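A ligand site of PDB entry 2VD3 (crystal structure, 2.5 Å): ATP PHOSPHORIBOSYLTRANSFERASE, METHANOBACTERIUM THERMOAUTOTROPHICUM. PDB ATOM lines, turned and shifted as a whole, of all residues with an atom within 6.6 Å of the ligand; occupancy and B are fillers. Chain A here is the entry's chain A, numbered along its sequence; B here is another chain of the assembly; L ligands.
The backbone carbonyl oxygen (O) of Leu 221 of chain B sits at hydrogen-bond distance from the backbone NH (N) of Val 255 of chain B, at 2.8 Å.
OG1 of Thr 239 lies within hydrogen-bond range of OD2 of Asp 278 of chain B.
The backbone NH (N) of Leu 280 of chain B is in hydrogen-bond range of the backbone carbonyl oxygen (O) of Met 220 of chain B (2.7 Å).
The side-chain amide nitrogen of Asn 222 of chain B lies within hydrogen-bond range of the side-chain hydroxyl of Thr 239, at 3.4 Å.
The side-chain amide nitrogen (ND2) of Asn 222 of chain B sits at hydrogen-bond distance from the side-chain carboxylate (OD2) of Asp 278 of chain B (2.9 Å).
O of Thr 242 lies within hydrogen-bond range of N of His 256 of chain A (2.8 Å).
OG1 of Thr 239 lies within hydrogen-bond range of NH2 of Arg 277 of chain B.
N of Asn 222 of chain B lies within hydrogen-bond range of O of Arg 277 of chain B (3.0 Å).
Residues that only touch the ligand: Gly 237, His 256 of chain A, Ala 257, Met 220 of chain B, Leu 221 of chain B and Leu 280 of chain B.
Within 4 Å of the ligand: Gly 237, Met 238, Thr 239, Gly 240, Thr 242, His 256 of chain A, Ala 257, Val 258, Met 220 of chain B, Leu 221 of chain B, Asn 222 of chain B, Asp 278 of chain B and Leu 280 of chain B.
The backbone NH of Met 238 sits at hydrogen-bond distance from an oxygen (O1) of the ligand, 2.8 Å away.
A nitrogen (N1) of the ligand lies within hydrogen-bond range of the side-chain hydroxyl (OG1) of Thr 242, at 2.6 Å.
An oxygen (O2) of the ligand is in hydrogen-bond range of the backbone NH (N) of Thr 239, 3.1 Å away.
The side-chain amide nitrogen of Asn 222 of chain B lies within hydrogen-bond range of an oxygen (O2) of the ligand (2.7 Å).
O of Asp 278 of chain B sits at hydrogen-bond distance from N3 of the ligand (3.0 Å).
The backbone NH (N) of Val 258 lies within hydrogen-bond range of an oxygen (O1) of the ligand (3.2 Å).
O of Gly 240 is in hydrogen-bond range of N1 of the ligand (2.8 Å).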
ATOM      1  N   LEU A 218      24.722  -8.568 -14.147  1.00  0.00           N
ATOM      2  CA  LEU A 218      25.918  -8.131 -13.427  1.00  0.00           C
ATOM      3  C   LEU A 218      26.995  -7.662 -14.411  1.00  0.00           C
ATOM      4  O   LEU A 218      27.575  -8.480 -15.141  1.00  0.00           O
ATOM      5  CB  LEU A 218      26.455  -9.245 -12.516  1.00  0.00           C
ATOM      6  CG  LEU A 218      27.748  -9.005 -11.723  1.00  0.00           C
ATOM      7  CD1 LEU A 218      27.523  -8.073 -10.557  1.00  0.00           C
ATOM      8  CD2 LEU A 218      28.349 -10.317 -11.231  1.00  0.00           C
ATOM      9  N   MET A 235      27.813   3.755 -12.328  1.00  0.00           N
ATOM     10  CA  MET A 235      27.365   2.451 -11.877  1.00  0.00           C
ATOM     11  C   MET A 235      27.045   2.468 -10.376  1.00  0.00           C
ATOM     12  O   MET A 235      27.827   1.934  -9.587  1.00  0.00           O
ATOM     13  CB  MET A 235      28.441   1.382 -12.147  1.00  0.00           C
ATOM     14  CG  MET A 235      28.817   1.201 -13.590  1.00  0.00           C
ATOM     15  SD  MET A 235      28.971  -0.546 -13.984  1.00  0.00           S
ATOM     16  CE  MET A 235      30.538  -0.985 -13.255  1.00  0.00           C
ATOM     17  N   PRO A 236      25.899   3.043  -9.977  1.00  0.00           N
ATOM     18  CA  PRO A 236      25.619   3.035  -8.534  1.00  0.00           C
ATOM     19  C   PRO A 236      25.361   1.611  -8.023  1.00  0.00           C
ATOM     20  O   PRO A 236      25.695   1.296  -6.885  1.00  0.00           O
ATOM     21  CB  PRO A 236      24.362   3.897  -8.404  1.00  0.00           C
ATOM     22  CG  PRO A 236      24.187   4.583  -9.736  1.00  0.00           C
ATOM     23  CD  PRO A 236      24.819   3.688 -10.734  1.00  0.00           C
ATOM     24  N   GLY A 237      24.790   0.762  -8.872  1.00  0.00           N
ATOM     25  CA  GLY A 237      24.473  -0.613  -8.490  1.00  0.00           C
ATOM     26  C   GLY A 237      23.452  -0.644  -7.367  1.00  0.00           C
ATOM     27  O   GLY A 237      22.638   0.272  -7.226  1.00  0.00           O
ATOM     28  N   MET A 238      23.502  -1.702  -6.563  1.00  0.00           N
ATOM     29  CA  MET A 238      22.492  -1.902  -5.534  1.00  0.00           C
ATOM     30  C   MET A 238      22.782  -1.127  -4.245  1.00  0.00           C
ATOM     31  O   MET A 238      21.903  -0.433  -3.747  1.00  0.00           O
ATOM     32  CB  MET A 238      22.220  -3.388  -5.315  1.00  0.00           C
ATOM     33  CG  MET A 238      21.005  -3.855  -6.108  1.00  0.00           C
ATOM     34  SD  MET A 238      20.837  -5.636  -6.357  1.00  0.00           S
ATOM     35  CE  MET A 238      19.190  -5.703  -7.056  1.00  0.00           C
ATOM     36  N   THR A 239      24.004  -1.234  -3.751  1.00  0.00           N
ATOM     37  CA  THR A 239      24.474  -0.404  -2.639  1.00  0.00           C
ATOM     38  C   THR A 239      25.592   0.523  -3.127  1.00  0.00           C
ATOM     39  O   THR A 239      25.718   1.662  -2.691  1.00  0.00           O
ATOM     40  CB  THR A 239      24.990  -1.275  -1.463  1.00  0.00           C
ATOM     41  OG1 THR A 239      23.938  -2.147  -1.025  1.00  0.00           O
ATOM     42  CG2 THR A 239      25.420  -0.421  -0.292  1.00  0.00           C
ATOM     43  N   GLY A 240      26.388   0.004  -4.055  1.00  0.00           N
ATOM     44  CA  GLY A 240      27.566   0.677  -4.603  1.00  0.00           C
ATOM     45  C   GLY A 240      28.408  -0.338  -5.357  1.00  0.00           C
ATOM     46  O   GLY A 240      28.364  -1.538  -5.048  1.00  0.00           O
ATOM     47  N   PRO A 241      29.182   0.138  -6.353  1.00  0.00           N
ATOM     48  CA  PRO A 241      29.994  -0.768  -7.183  1.00  0.00           C
ATOM     49  C   PRO A 241      31.055  -1.484  -6.364  1.00  0.00           C
ATOM     50  O   PRO A 241      31.624  -0.912  -5.437  1.00  0.00           O
ATOM     51  CB  PRO A 241      30.664   0.184  -8.186  1.00  0.00           C
ATOM     52  CG  PRO A 241      30.623   1.522  -7.543  1.00  0.00           C
ATOM     53  CD  PRO A 241      29.352   1.543  -6.752  1.00  0.00           C
ATOM     54  N   THR A 242      31.302  -2.747  -6.716  1.00  0.00           N
ATOM     55  CA  THR A 242      32.340  -3.538  -6.065  1.00  0.00           C
ATOM     56  C   THR A 242      33.625  -3.364  -6.846  1.00  0.00           C
ATOM     57  O   THR A 242      33.646  -3.538  -8.074  1.00  0.00           O
ATOM     58  CB  THR A 242      31.943  -5.045  -5.980  1.00  0.00           C
ATOM     59  OG1 THR A 242      30.686  -5.193  -5.319  1.00  0.00           O
ATOM     60  CG2 THR A 242      32.992  -5.834  -5.222  1.00  0.00           C
ATOM     61  N   HIS A 256      32.484  -4.081 -10.519  1.00  0.00           N
ATOM     62  CA  HIS A 256      31.254  -4.836 -10.801  1.00  0.00           C
ATOM     63  C   HIS A 256      30.018  -4.164 -10.161  1.00  0.00           C
ATOM     64  O   HIS A 256      30.092  -3.720  -9.008  1.00  0.00           O
ATOM     65  CB  HIS A 256      31.354  -6.291 -10.302  1.00  0.00           C
ATOM     66  CG  HIS A 256      32.731  -6.898 -10.434  1.00  0.00           C
ATOM     67  ND1 HIS A 256      33.253  -7.739  -9.478  1.00  0.00           N
ATOM     68  CD2 HIS A 256      33.672  -6.792 -11.393  1.00  0.00           C
ATOM     69  CE1 HIS A 256      34.457  -8.127  -9.857  1.00  0.00           C
ATOM     70  NE2 HIS A 256      34.739  -7.564 -11.013  1.00  0.00           N
ATOM     71  N   ALA A 257      28.910  -4.136 -10.886  1.00  0.00           N
ATOM     72  CA  ALA A 257      27.646  -3.613 -10.383  1.00  0.00           C
ATOM     73  C   ALA A 257      26.483  -4.295 -11.090  1.00  0.00           C
ATOM     74  O   ALA A 257      26.576  -4.637 -12.274  1.00  0.00           O
ATOM     75  CB  ALA A 257      27.573  -2.111 -10.575  1.00  0.00           C
ATOM     76  N   VAL A 258      25.403  -4.498 -10.340  1.00  0.00           N
ATOM     77  CA  VAL A 258      24.152  -4.978 -10.913  1.00  0.00           C
ATOM     78  C   VAL A 258      23.527  -3.807 -11.671  1.00  0.00           C
ATOM     79  O   VAL A 258      23.425  -2.689 -11.137  1.00  0.00           O
ATOM     80  CB  VAL A 258      23.179  -5.478  -9.814  1.00  0.00           C
ATOM     81  CG1 VAL A 258      21.933  -6.091 -10.436  1.00  0.00           C
ATOM     82  CG2 VAL A 258      23.877  -6.466  -8.880  1.00  0.00           C
ATOM     83  N   VAL A 259      23.166  -4.019 -12.939  1.00  0.00           N
ATOM     84  CA  VAL A 259      22.560  -2.959 -13.728  1.00  0.00           C
ATOM     85  C   VAL A 259      21.299  -3.453 -14.449  1.00  0.00           C
ATOM     86  O   VAL A 259      21.223  -4.605 -14.859  1.00  0.00           O
ATOM     87  CB  VAL A 259      23.563  -2.286 -14.730  1.00  0.00           C
ATOM     88  CG1 VAL A 259      24.990  -2.307 -14.176  1.00  0.00           C
ATOM     89  CG2 VAL A 259      23.523  -2.949 -16.082  1.00  0.00           C
ATOM     90  N   MET B 220      26.286 -14.000  -4.032  1.00  0.00           N
ATOM     91  CA  MET B 220      26.920 -12.710  -3.755  1.00  0.00           C
ATOM     92  C   MET B 220      25.997 -11.820  -2.926  1.00  0.00           C
ATOM     93  O   MET B 220      24.774 -11.844  -3.123  1.00  0.00           O
ATOM     94  CB  MET B 220      27.266 -11.975  -5.054  1.00  0.00           C
ATOM     95  CG  MET B 220      28.154 -12.725  -6.013  1.00  0.00           C
ATOM     96  SD  MET B 220      28.100 -12.059  -7.684  1.00  0.00           S
ATOM     97  CE  MET B 220      29.293 -10.730  -7.615  1.00  0.00           C
ATOM     98  N   LEU B 221      26.589 -11.027  -2.037  1.00  0.00           N
ATOM     99  CA  LEU B 221      25.821 -10.124  -1.168  1.00  0.00           C
ATOM    100  C   LEU B 221      26.633  -8.909  -0.736  1.00  0.00           C
ATOM    101  O   LEU B 221      27.857  -8.952  -0.674  1.00  0.00           O
ATOM    102  CB  LEU B 221      25.288 -10.859   0.065  1.00  0.00           C
ATOM    103  CG  LEU B 221      26.253 -11.585   1.017  1.00  0.00           C
ATOM    104  CD1 LEU B 221      27.020 -10.630   1.953  1.00  0.00           C
ATOM    105  CD2 LEU B 221      25.477 -12.573   1.842  1.00  0.00           C
ATOM    106  N   ASN B 222      25.919  -7.828  -0.434  1.00  0.00           N
ATOM    107  CA  ASN B 222      26.511  -6.646   0.183  1.00  0.00           C
ATOM    108  C   ASN B 222      26.250  -6.650   1.688  1.00  0.00           C
ATOM    109  O   ASN B 222      25.103  -6.782   2.127  1.00  0.00           O
ATOM    110  CB  ASN B 222      25.947  -5.377  -0.450  1.00  0.00           C
ATOM    111  CG  ASN B 222      26.375  -5.193  -1.895  1.00  0.00           C
ATOM    112  OD1 ASN B 222      27.502  -5.536  -2.279  1.00  0.00           O
ATOM    113  ND2 ASN B 222      25.491  -4.634  -2.712  1.00  0.00           N
ATOM    114  N   GLU B 245      35.774  -4.764  -1.611  1.00  0.00           N
ATOM    115  CA  GLU B 245      35.352  -3.446  -1.162  1.00  0.00           C
ATOM    116  C   GLU B 245      34.165  -2.967  -1.987  1.00  0.00           C
ATOM    117  O   GLU B 245      34.060  -3.263  -3.178  1.00  0.00           O
ATOM    118  CB  GLU B 245      36.512  -2.444  -1.263  1.00  0.00           C
ATOM    119  CG  GLU B 245      36.317  -1.122  -0.523  1.00  0.00           C
ATOM    120  CD  GLU B 245      36.600  -1.210   0.978  1.00  0.00           C
ATOM    121  OE1 GLU B 245      36.232  -0.254   1.719  1.00  0.00           O
ATOM    122  OE2 GLU B 245      37.196  -2.209   1.438  1.00  0.00           O
ATOM    123  N   VAL B 246      33.263  -2.230  -1.327  1.00  0.00           N
ATOM    124  CA  VAL B 246      32.136  -1.577  -1.987  1.00  0.00           C
ATOM    125  C   VAL B 246      32.251  -0.078  -1.754  1.00  0.00           C
ATOM    126  O   VAL B 246      32.440   0.360  -0.619  1.00  0.00           O
ATOM    127  CB  VAL B 246      30.782  -2.119  -1.473  1.00  0.00           C
ATOM    128  CG1 VAL B 246      29.610  -1.281  -1.980  1.00  0.00           C
ATOM    129  CG2 VAL B 246      30.597  -3.566  -1.877  1.00  0.00           C
ATOM    130  N   ALA B 254      31.532  -6.655  -0.160  1.00  0.00           N
ATOM    131  CA  ALA B 254      30.789  -7.611  -0.970  1.00  0.00           C
ATOM    132  C   ALA B 254      31.372  -8.997  -0.703  1.00  0.00           C
ATOM    133  O   ALA B 254      32.595  -9.154  -0.697  1.00  0.00           O
ATOM    134  CB  ALA B 254      30.879  -7.273  -2.442  1.00  0.00           C
ATOM    135  N   VAL B 255      30.511  -9.966  -0.466  1.00  0.00           N
ATOM    136  CA  VAL B 255      30.964 -11.304  -0.113  1.00  0.00           C
ATOM    137  C   VAL B 255      30.406 -12.311  -1.100  1.00  0.00           C
ATOM    138  O   VAL B 255      29.196 -12.340  -1.341  1.00  0.00           O
ATOM    139  CB  VAL B 255      30.521 -11.696   1.318  1.00  0.00           C
ATOM    140  CG1 VAL B 255      31.051 -13.064   1.695  1.00  0.00           C
ATOM    141  CG2 VAL B 255      30.960 -10.661   2.329  1.00  0.00           C
ATOM    142  N   HIS B 256      31.290 -13.117  -1.699  1.00  0.00           N
ATOM    143  CA  HIS B 256      30.876 -14.179  -2.630  1.00  0.00           C
ATOM    144  C   HIS B 256      31.323 -15.563  -2.149  1.00  0.00           C
ATOM    145  O   HIS B 256      32.456 -15.709  -1.676  1.00  0.00           O
ATOM    146  CB  HIS B 256      31.434 -13.926  -4.055  1.00  0.00           C
ATOM    147  CG  HIS B 256      31.507 -12.479  -4.449  1.00  0.00           C
ATOM    148  ND1 HIS B 256      32.546 -11.962  -5.192  1.00  0.00           N
ATOM    149  CD2 HIS B 256      30.670 -11.439  -4.214  1.00  0.00           C
ATOM    150  CE1 HIS B 256      32.340 -10.676  -5.399  1.00  0.00           C
ATOM    151  NE2 HIS B 256      31.215 -10.332  -4.816  1.00  0.00           N
ATOM    152  N   ARG B 277      22.207  -7.616   2.304  1.00  0.00           N
ATOM    153  CA  ARG B 277      21.265  -7.158   1.277  1.00  0.00           C
ATOM    154  C   ARG B 277      21.789  -7.466  -0.122  1.00  0.00           C
ATOM    155  O   ARG B 277      22.950  -7.871  -0.286  1.00  0.00           O
ATOM    156  CB  ARG B 277      20.905  -5.665   1.460  1.00  0.00           C
ATOM    157  CG  ARG B 277      22.068  -4.704   1.680  1.00  0.00           C
ATOM    158  CD  ARG B 277      21.567  -3.440   2.381  1.00  0.00           C
ATOM    159  NE  ARG B 277      22.645  -2.606   2.920  1.00  0.00           N
ATOM    160  CZ  ARG B 277      23.006  -1.427   2.429  1.00  0.00           C
ATOM    161  NH1 ARG B 277      24.004  -0.746   2.996  1.00  0.00           N
ATOM    162  NH2 ARG B 277      22.388  -0.915   1.375  1.00  0.00           N
ATOM    163  N   ASP B 278      20.916  -7.288  -1.114  1.00  0.00           N
ATOM    164  CA  ASP B 278      21.247  -7.451  -2.540  1.00  0.00           C
ATOM    165  C   ASP B 278      21.822  -8.826  -2.854  1.00  0.00           C
ATOM    166  O   ASP B 278      22.859  -8.954  -3.521  1.00  0.00           O
ATOM    167  CB  ASP B 278      22.203  -6.342  -2.998  1.00  0.00           C
ATOM    168  CG  ASP B 278      21.860  -4.998  -2.404  1.00  0.00           C
ATOM    169  OD1 ASP B 278      20.688  -4.611  -2.451  1.00  0.00           O
ATOM    170  OD2 ASP B 278      22.779  -4.337  -1.869  1.00  0.00           O
ATOM    171  N   ILE B 279      21.143  -9.862  -2.370  1.00  0.00           N
ATOM    172  CA  ILE B 279      21.617 -11.225  -2.532  1.00  0.00           C
ATOM    173  C   ILE B 279      21.410 -11.717  -3.960  1.00  0.00           C
ATOM    174  O   ILE B 279      20.282 -11.764  -4.465  1.00  0.00           O
ATOM    175  CB  ILE B 279      20.984 -12.188  -1.510  1.00  0.00           C
ATOM    176  CG1 ILE B 279      21.116 -11.627  -0.091  1.00  0.00           C
ATOM    177  CG2 ILE B 279      21.643 -13.566  -1.625  1.00  0.00           C
ATOM    178  CD1 ILE B 279      20.231 -12.338   0.933  1.00  0.00           C
ATOM    179  N   LEU B 280      22.516 -12.064  -4.605  1.00  0.00           N
ATOM    180  CA  LEU B 280      22.518 -12.516  -5.974  1.00  0.00           C
ATOM    181  C   LEU B 280      22.876 -13.978  -6.011  1.00  0.00           C
ATOM    182  O   LEU B 280      23.755 -14.434  -5.257  1.00  0.00           O
ATOM    183  CB  LEU B 280      23.521 -11.737  -6.825  1.00  0.00           C
ATOM    184  CG  LEU B 280      23.741 -10.238  -6.589  1.00  0.00           C
ATOM    185  CD1 LEU B 280      24.786  -9.742  -7.559  1.00  0.00           C
ATOM    186  CD2 LEU B 280      22.447  -9.427  -6.700  1.00  0.00           C
HETATM  187  N1  LIG L   1      28.217  -4.319  -5.070  1.00  0.00           N
HETATM  188  C1  LIG L   1      27.460  -4.454  -6.356  1.00  0.00           C
HETATM  189  C2  LIG L   1      26.062  -3.852  -6.264  1.00  0.00           C
HETATM  190  O1  LIG L   1      25.386  -3.672  -7.269  1.00  0.00           O
HETATM  191  C3  LIG L   1      27.360  -5.928  -6.780  1.00  0.00           C
HETATM  192  C4  LIG L   1      26.766  -6.814  -5.729  1.00  0.00           C
HETATM  193  N2  LIG L   1      27.489  -7.812  -5.103  1.00  0.00           N
HETATM  194  C5  LIG L   1      25.520  -6.863  -5.196  1.00  0.00           C
HETATM  195  C6  LIG L   1      26.712  -8.431  -4.225  1.00  0.00           C
HETATM  196  N3  LIG L   1      25.514  -7.868  -4.271  1.00  0.00           N
HETATM  197  O2  LIG L   1      25.577  -3.545  -5.162  1.00  0.00           O
